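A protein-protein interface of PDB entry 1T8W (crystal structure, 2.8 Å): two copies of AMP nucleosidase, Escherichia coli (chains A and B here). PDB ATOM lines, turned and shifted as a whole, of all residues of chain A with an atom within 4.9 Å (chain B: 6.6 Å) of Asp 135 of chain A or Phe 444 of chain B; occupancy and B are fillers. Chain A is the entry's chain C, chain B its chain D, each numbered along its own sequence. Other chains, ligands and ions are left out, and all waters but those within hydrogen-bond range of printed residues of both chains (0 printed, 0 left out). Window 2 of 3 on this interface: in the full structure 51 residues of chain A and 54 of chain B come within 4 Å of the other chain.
The guanidinium group of Arg 443 of chain B lies within hydrogen-bond range of the backbone carbonyl oxygen of Leu 134 of chain A. NH1 of Arg 136 of chain A sits at hydrogen-bond distance from O of Ile 315 of chain B (3.3 Å).
OD1 of Asp 135 of chain A lies within hydrogen-bond range of N of Met 138 of chain A (3.1 Å). The side-chain carboxylate (OD1) of Asp 135 of chain A is in hydrogen-bond range of the backbone NH (N) of Ser 137 of chain A (2.8 Å). The backbone carbonyl oxygen of Asp 135 of chain A sits at hydrogen-bond distance from the side-chain hydroxyl of Ser 139 of chain A (2.8 Å).
Among the printed residues, merely in contact across the chains: Arg 136 of chain A with Phe 444 of chain B (3.0 Å), Leu 134 of chain A with Phe 444 of chain B (3.2 Å), Asp 135 of chain A with Phe 444 of chain B (3.6 Å) and Thr 133 of chain A with Arg 443 of chain B (3.98 Å).
Printed residues of chain B within 4 Å of Thr 133 of chain A: Arg 443 (3.98 Å). Of the printed residues of chain B, Leu 134 of chain A touches Arg 443 (3.5 Å) and Phe 444 (3.2 Å). Asp 135 of chain A touches one residue of chain B. Of the printed residues of chain B, Arg 136 of chain A touches Ile 315 (3.3 Å) and Phe 444 (3.0 Å). Of the printed residues of chain A, Ile 315 of chain B touches Arg 136. Printed residues of chain A within 4 Å of Arg 443 of chain B: Thr 133 (3.98 Å) and Leu 134 (3.5 Å). Phe 444 of chain B touches just these residues of chain A: Leu 134 (3.2 Å), Asp 135 (3.6 Å) and Arg 136 (3.0 Å). The nearest residue of chain A that does not touch Phe 444 of chain B is Ser 139 of chain A (4.5 Å). The nearest printed residue of chain B that does not touch Arg 136 of chain A is Gly 316 of chain B (5.2 Å).
Hydrophobic or aromatic side chains of chain B that line the printed part of chain A: Phe 444. Of the 7 printed residues of chain A, 4 touch a printed residue of chain B. Among the printed residues, 6 pairs touch across the chains. Among the printed residues, no Asp or Glu carboxylate lies within 4 Å of a Lys or Arg side-chain nitrogen of the other chain.
No position is printed for both chains. Of the 6 pairs that touch across the chains among the printed residues, none has its exchanged pair printed and touching as well.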
ATOM      1  N   THR A 133       9.817 -23.397  -3.441  1.00  0.00           N
ATOM      2  CA  THR A 133       8.444 -23.839  -3.275  1.00  0.00           C
ATOM      3  C   THR A 133       8.472 -25.188  -2.589  1.00  0.00           C
ATOM      4  O   THR A 133       7.789 -26.105  -3.045  1.00  0.00           O
ATOM      5  CB  THR A 133       7.718 -24.024  -4.638  1.00  0.00           C
ATOM      6  OG1 THR A 133       8.191 -23.054  -5.578  1.00  0.00           O
ATOM      7  CG2 THR A 133       6.207 -23.852  -4.470  1.00  0.00           C
ATOM      8  N   LEU A 134       9.231 -25.363  -1.506  1.00  0.00           N
ATOM      9  CA  LEU A 134       9.172 -26.708  -0.991  1.00  0.00           C
ATOM     10  C   LEU A 134       8.016 -26.944  -0.048  1.00  0.00           C
ATOM     11  O   LEU A 134       7.690 -26.114   0.799  1.00  0.00           O
ATOM     12  CB  LEU A 134      10.509 -27.141  -0.380  1.00  0.00           C
ATOM     13  CG  LEU A 134      11.579 -27.384  -1.457  1.00  0.00           C
ATOM     14  CD1 LEU A 134      12.100 -26.050  -1.974  1.00  0.00           C
ATOM     15  CD2 LEU A 134      12.713 -28.210  -0.882  1.00  0.00           C
ATOM     16  N   ASP A 135       7.364 -28.079  -0.248  1.00  0.00           N
ATOM     17  CA  ASP A 135       6.235 -28.474   0.569  1.00  0.00           C
ATOM     18  C   ASP A 135       6.759 -29.185   1.813  1.00  0.00           C
ATOM     19  O   ASP A 135       7.964 -29.238   2.057  1.00  0.00           O
ATOM     20  CB  ASP A 135       5.332 -29.422  -0.217  1.00  0.00           C
ATOM     21  CG  ASP A 135       6.034 -30.724  -0.586  1.00  0.00           C
ATOM     22  OD1 ASP A 135       6.317 -31.535   0.327  1.00  0.00           O
ATOM     23  OD2 ASP A 135       6.310 -30.930  -1.789  1.00  0.00           O
ATOM     24  N   ARG A 136       5.838 -29.742   2.587  1.00  0.00           N
ATOM     25  CA  ARG A 136       6.182 -30.449   3.808  1.00  0.00           C
ATOM     26  C   ARG A 136       7.290 -31.477   3.626  1.00  0.00           C
ATOM     27  O   ARG A 136       8.385 -31.316   4.171  1.00  0.00           O
ATOM     28  CB  ARG A 136       4.941 -31.143   4.370  1.00  0.00           C
ATOM     29  CG  ARG A 136       3.833 -30.188   4.769  1.00  0.00           C
ATOM     30  CD  ARG A 136       4.255 -29.319   5.935  1.00  0.00           C
ATOM     31  NE  ARG A 136       3.204 -28.386   6.317  1.00  0.00           N
ATOM     32  CZ  ARG A 136       3.294 -27.528   7.326  1.00  0.00           C
ATOM     33  NH1 ARG A 136       4.395 -27.477   8.071  1.00  0.00           N
ATOM     34  NH2 ARG A 136       2.286 -26.707   7.580  1.00  0.00           N
ATOM     35  N   SER A 137       6.994 -32.533   2.868  1.00  0.00           N
ATOM     36  CA  SER A 137       7.943 -33.621   2.616  1.00  0.00           C
ATOM     37  C   SER A 137       9.286 -33.119   2.125  1.00  0.00           C
ATOM     38  O   SER A 137      10.336 -33.540   2.613  1.00  0.00           O
ATOM     39  CB  SER A 137       7.378 -34.601   1.584  1.00  0.00           C
ATOM     40  OG  SER A 137       6.193 -35.210   2.058  1.00  0.00           O
ATOM     41  N   MET A 138       9.241 -32.228   1.142  1.00  0.00           N
ATOM     42  CA  MET A 138      10.453 -31.657   0.569  1.00  0.00           C
ATOM     43  C   MET A 138      11.357 -31.090   1.657  1.00  0.00           C
ATOM     44  O   MET A 138      12.549 -31.410   1.732  1.00  0.00           O
ATOM     45  CB  MET A 138      10.081 -30.555  -0.427  1.00  0.00           C
ATOM     46  CG  MET A 138       9.573 -31.085  -1.760  1.00  0.00           C
ATOM     47  SD  MET A 138      10.980 -32.070  -2.686  1.00  0.00           S
ATOM     48  CE  MET A 138      11.727 -30.576  -3.692  1.00  0.00           C
ATOM     49  N   SER A 139      10.771 -30.248   2.502  1.00  0.00           N
ATOM     50  CA  SER A 139      11.488 -29.617   3.597  1.00  0.00           C
ATOM     51  C   SER A 139      12.028 -30.656   4.565  1.00  0.00           C
ATOM     52  O   SER A 139      13.233 -30.704   4.826  1.00  0.00           O
ATOM     53  CB  SER A 139      10.556 -28.665   4.336  1.00  0.00           C
ATOM     54  OG  SER A 139       9.977 -27.759   3.422  1.00  0.00           O
ATOM     55  N   ILE B 315       5.874 -26.126  11.915  1.00  0.00           N
ATOM     56  CA  ILE B 315       5.696 -24.708  11.636  1.00  0.00           C
ATOM     57  C   ILE B 315       4.265 -24.501  11.192  1.00  0.00           C
ATOM     58  O   ILE B 315       3.788 -25.190  10.302  1.00  0.00           O
ATOM     59  CB  ILE B 315       6.635 -24.225  10.523  1.00  0.00           C
ATOM     60  CG1 ILE B 315       8.073 -24.211  11.054  1.00  0.00           C
ATOM     61  CG2 ILE B 315       6.169 -22.866   9.999  1.00  0.00           C
ATOM     62  CD1 ILE B 315       9.084 -23.626  10.096  1.00  0.00           C
ATOM     63  N   GLY B 316       3.579 -23.564  11.828  1.00  0.00           N
ATOM     64  CA  GLY B 316       2.199 -23.292  11.481  1.00  0.00           C
ATOM     65  C   GLY B 316       1.264 -23.715  12.592  1.00  0.00           C
ATOM     66  O   GLY B 316       0.119 -23.250  12.651  1.00  0.00           O
ATOM     67  N   ARG B 369      -2.859 -29.776  15.865  1.00  0.00           N
ATOM     68  CA  ARG B 369      -2.497 -28.475  15.345  1.00  0.00           C
ATOM     69  C   ARG B 369      -2.260 -27.513  16.521  1.00  0.00           C
ATOM     70  O   ARG B 369      -1.470 -26.576  16.418  1.00  0.00           O
ATOM     71  CB  ARG B 369      -3.629 -27.975  14.440  1.00  0.00           C
ATOM     72  CG  ARG B 369      -3.314 -26.726  13.642  1.00  0.00           C
ATOM     73  CD  ARG B 369      -2.371 -27.004  12.471  1.00  0.00           C
ATOM     74  NE  ARG B 369      -1.912 -25.767  11.830  1.00  0.00           N
ATOM     75  CZ  ARG B 369      -2.717 -24.859  11.277  1.00  0.00           C
ATOM     76  NH1 ARG B 369      -4.032 -25.046  11.278  1.00  0.00           N
ATOM     77  NH2 ARG B 369      -2.209 -23.754  10.735  1.00  0.00           N
ATOM     78  N   CYS B 425       1.681 -18.673  17.210  1.00  0.00           N
ATOM     79  CA  CYS B 425       1.742 -19.534  16.039  1.00  0.00           C
ATOM     80  C   CYS B 425       3.211 -19.851  15.804  1.00  0.00           C
ATOM     81  O   CYS B 425       4.022 -18.933  15.678  1.00  0.00           O
ATOM     82  CB  CYS B 425       1.152 -18.803  14.832  1.00  0.00           C
ATOM     83  SG  CYS B 425       1.083 -19.782  13.350  1.00  0.00           S
ATOM     84  N   VAL B 426       3.554 -21.138  15.751  1.00  0.00           N
ATOM     85  CA  VAL B 426       4.944 -21.550  15.558  1.00  0.00           C
ATOM     86  C   VAL B 426       5.484 -21.061  14.223  1.00  0.00           C
ATOM     87  O   VAL B 426       5.005 -21.476  13.183  1.00  0.00           O
ATOM     88  CB  VAL B 426       5.085 -23.076  15.614  1.00  0.00           C
ATOM     89  CG1 VAL B 426       6.546 -23.444  15.519  1.00  0.00           C
ATOM     90  CG2 VAL B 426       4.479 -23.618  16.914  1.00  0.00           C
ATOM     91  N   LYS B 436      14.291 -19.995  11.325  1.00  0.00           N
ATOM     92  CA  LYS B 436      13.813 -18.972  10.400  1.00  0.00           C
ATOM     93  C   LYS B 436      13.675 -17.628  11.124  1.00  0.00           C
ATOM     94  O   LYS B 436      14.069 -17.490  12.288  1.00  0.00           O
ATOM     95  CB  LYS B 436      12.451 -19.387   9.827  1.00  0.00           C
ATOM     96  CG  LYS B 436      12.257 -20.900   9.690  1.00  0.00           C
ATOM     97  CD  LYS B 436      13.050 -21.497   8.534  1.00  0.00           C
ATOM     98  CE  LYS B 436      12.336 -21.292   7.200  1.00  0.00           C
ATOM     99  NZ  LYS B 436      11.039 -22.033   7.132  1.00  0.00           N
ATOM    100  N   ALA B 441      11.526 -15.409   4.160  1.00  0.00           N
ATOM    101  CA  ALA B 441      10.774 -16.342   3.315  1.00  0.00           C
ATOM    102  C   ALA B 441      10.379 -17.615   4.060  1.00  0.00           C
ATOM    103  O   ALA B 441      11.120 -18.604   4.088  1.00  0.00           O
ATOM    104  CB  ALA B 441      11.589 -16.696   2.082  1.00  0.00           C
ATOM    105  N   ASN B 442       9.193 -17.583   4.657  1.00  0.00           N
ATOM    106  CA  ASN B 442       8.700 -18.714   5.417  1.00  0.00           C
ATOM    107  C   ASN B 442       7.355 -19.170   4.873  1.00  0.00           C
ATOM    108  O   ASN B 442       6.331 -19.036   5.537  1.00  0.00           O
ATOM    109  CB  ASN B 442       8.553 -18.319   6.881  1.00  0.00           C
ATOM    110  CG  ASN B 442       8.563 -19.511   7.793  1.00  0.00           C
ATOM    111  OD1 ASN B 442       8.343 -20.647   7.355  1.00  0.00           O
ATOM    112  ND2 ASN B 442       8.811 -19.269   9.073  1.00  0.00           N
ATOM    113  N   ARG B 443       7.371 -19.706   3.658  1.00  0.00           N
ATOM    114  CA  ARG B 443       6.166 -20.189   2.996  1.00  0.00           C
ATOM    115  C   ARG B 443       5.065 -20.684   3.948  1.00  0.00           C
ATOM    116  O   ARG B 443       3.918 -20.233   3.861  1.00  0.00           O
ATOM    117  CB  ARG B 443       6.533 -21.315   2.016  1.00  0.00           C
ATOM    118  CG  ARG B 443       5.976 -21.140   0.599  1.00  0.00           C
ATOM    119  CD  ARG B 443       6.269 -22.362  -0.284  1.00  0.00           C
ATOM    120  NE  ARG B 443       5.489 -23.539   0.108  1.00  0.00           N
ATOM    121  CZ  ARG B 443       4.195 -23.715  -0.162  1.00  0.00           C
ATOM    122  NH1 ARG B 443       3.517 -22.793  -0.836  1.00  0.00           N
ATOM    123  NH2 ARG B 443       3.576 -24.817   0.248  1.00  0.00           N
ATOM    124  N   PHE B 444       5.410 -21.590   4.864  1.00  0.00           N
ATOM    125  CA  PHE B 444       4.417 -22.152   5.781  1.00  0.00           C
ATOM    126  C   PHE B 444       3.870 -21.271   6.881  1.00  0.00           C
ATOM    127  O   PHE B 444       2.687 -21.337   7.203  1.00  0.00           O
ATOM    128  CB  PHE B 444       4.938 -23.456   6.369  1.00  0.00           C
ATOM    129  CG  PHE B 444       4.990 -24.554   5.366  1.00  0.00           C
ATOM    130  CD1 PHE B 444       6.036 -24.626   4.450  1.00  0.00           C
ATOM    131  CD2 PHE B 444       3.933 -25.452   5.252  1.00  0.00           C
ATOM    132  CE1 PHE B 444       6.029 -25.575   3.423  1.00  0.00           C
ATOM    133  CE2 PHE B 444       3.913 -26.406   4.230  1.00  0.00           C
ATOM    134  CZ  PHE B 444       4.965 -26.466   3.312  1.00  0.00           C
ATOM    135  N   TYR B 445       4.719 -20.454   7.476  1.00  0.00           N
ATOM    136  CA  TYR B 445       4.234 -19.576   8.512  1.00  0.00           C
ATOM    137  C   TYR B 445       3.348 -18.533   7.833  1.00  0.00           C
ATOM    138  O   TYR B 445       2.182 -18.388   8.188  1.00  0.00           O
ATOM    139  CB  TYR B 445       5.403 -18.916   9.263  1.00  0.00           C
ATOM    140  CG  TYR B 445       4.962 -17.836  10.223  1.00  0.00           C
ATOM    141  CD1 TYR B 445       4.063 -18.118  11.261  1.00  0.00           C
ATOM    142  CD2 TYR B 445       5.371 -16.517  10.045  1.00  0.00           C
ATOM    143  CE1 TYR B 445       3.579 -17.111  12.080  1.00  0.00           C
ATOM    144  CE2 TYR B 445       4.891 -15.505  10.860  1.00  0.00           C
ATOM    145  CZ  TYR B 445       3.997 -15.808  11.870  1.00  0.00           C
ATOM    146  OH  TYR B 445       3.518 -14.795  12.659  1.00  0.00           O
ATOM    147  N   GLU B 446       3.892 -17.835   6.839  1.00  0.00           N
ATOM    148  CA  GLU B 446       3.146 -16.805   6.110  1.00  0.00           C
ATOM    149  C   GLU B 446       1.738 -17.254   5.727  1.00  0.00           C
ATOM    150  O   GLU B 446       0.808 -16.443   5.675  1.00  0.00           O
ATOM    151  CB  GLU B 446       3.872 -16.418   4.821  1.00  0.00           C
ATOM    152  CG  GLU B 446       5.267 -15.870   4.994  1.00  0.00           C
ATOM    153  CD  GLU B 446       5.293 -14.504   5.648  1.00  0.00           C
ATOM    154  OE1 GLU B 446       4.528 -13.614   5.202  1.00  0.00           O
ATOM    155  OE2 GLU B 446       6.092 -14.323   6.602  1.00  0.00           O
ATOM    156  N   GLY B 447       1.595 -18.545   5.436  1.00  0.00           N
ATOM    157  CA  GLY B 447       0.307 -19.074   5.046  1.00  0.00           C
ATOM    158  C   GLY B 447      -0.683 -19.160   6.187  1.00  0.00           C
ATOM    159  O   GLY B 447      -1.893 -19.055   5.977  1.00  0.00           O
ATOM    160  N   ALA B 448      -0.168 -19.344   7.402  1.00  0.00           N
ATOM    161  CA  ALA B 448      -1.004 -19.466   8.591  1.00  0.00           C
ATOM    162  C   ALA B 448      -1.500 -18.130   9.146  1.00  0.00           C
ATOM    163  O   ALA B 448      -2.569 -18.065   9.756  1.00  0.00           O
ATOM    164  CB  ALA B 448      -0.242 -20.225   9.665  1.00  0.00           C
ATOM    165  N   ILE B 449      -0.735 -17.068   8.907  1.00  0.00           N
ATOM    166  CA  ILE B 449      -1.058 -15.740   9.419  1.00  0.00           C
ATOM    167  C   ILE B 449      -2.514 -15.310   9.408  1.00  0.00           C
ATOM    168  O   ILE B 449      -3.046 -14.921  10.450  1.00  0.00           O
ATOM    169  CB  ILE B 449      -0.187 -14.663   8.728  1.00  0.00           C
ATOM    170  CG1 ILE B 449       1.245 -14.774   9.271  1.00  0.00           C
ATOM    171  CG2 ILE B 449      -0.736 -13.258   8.994  1.00  0.00           C
ATOM    172  CD1 ILE B 449       2.245 -13.889   8.587  1.00  0.00           C
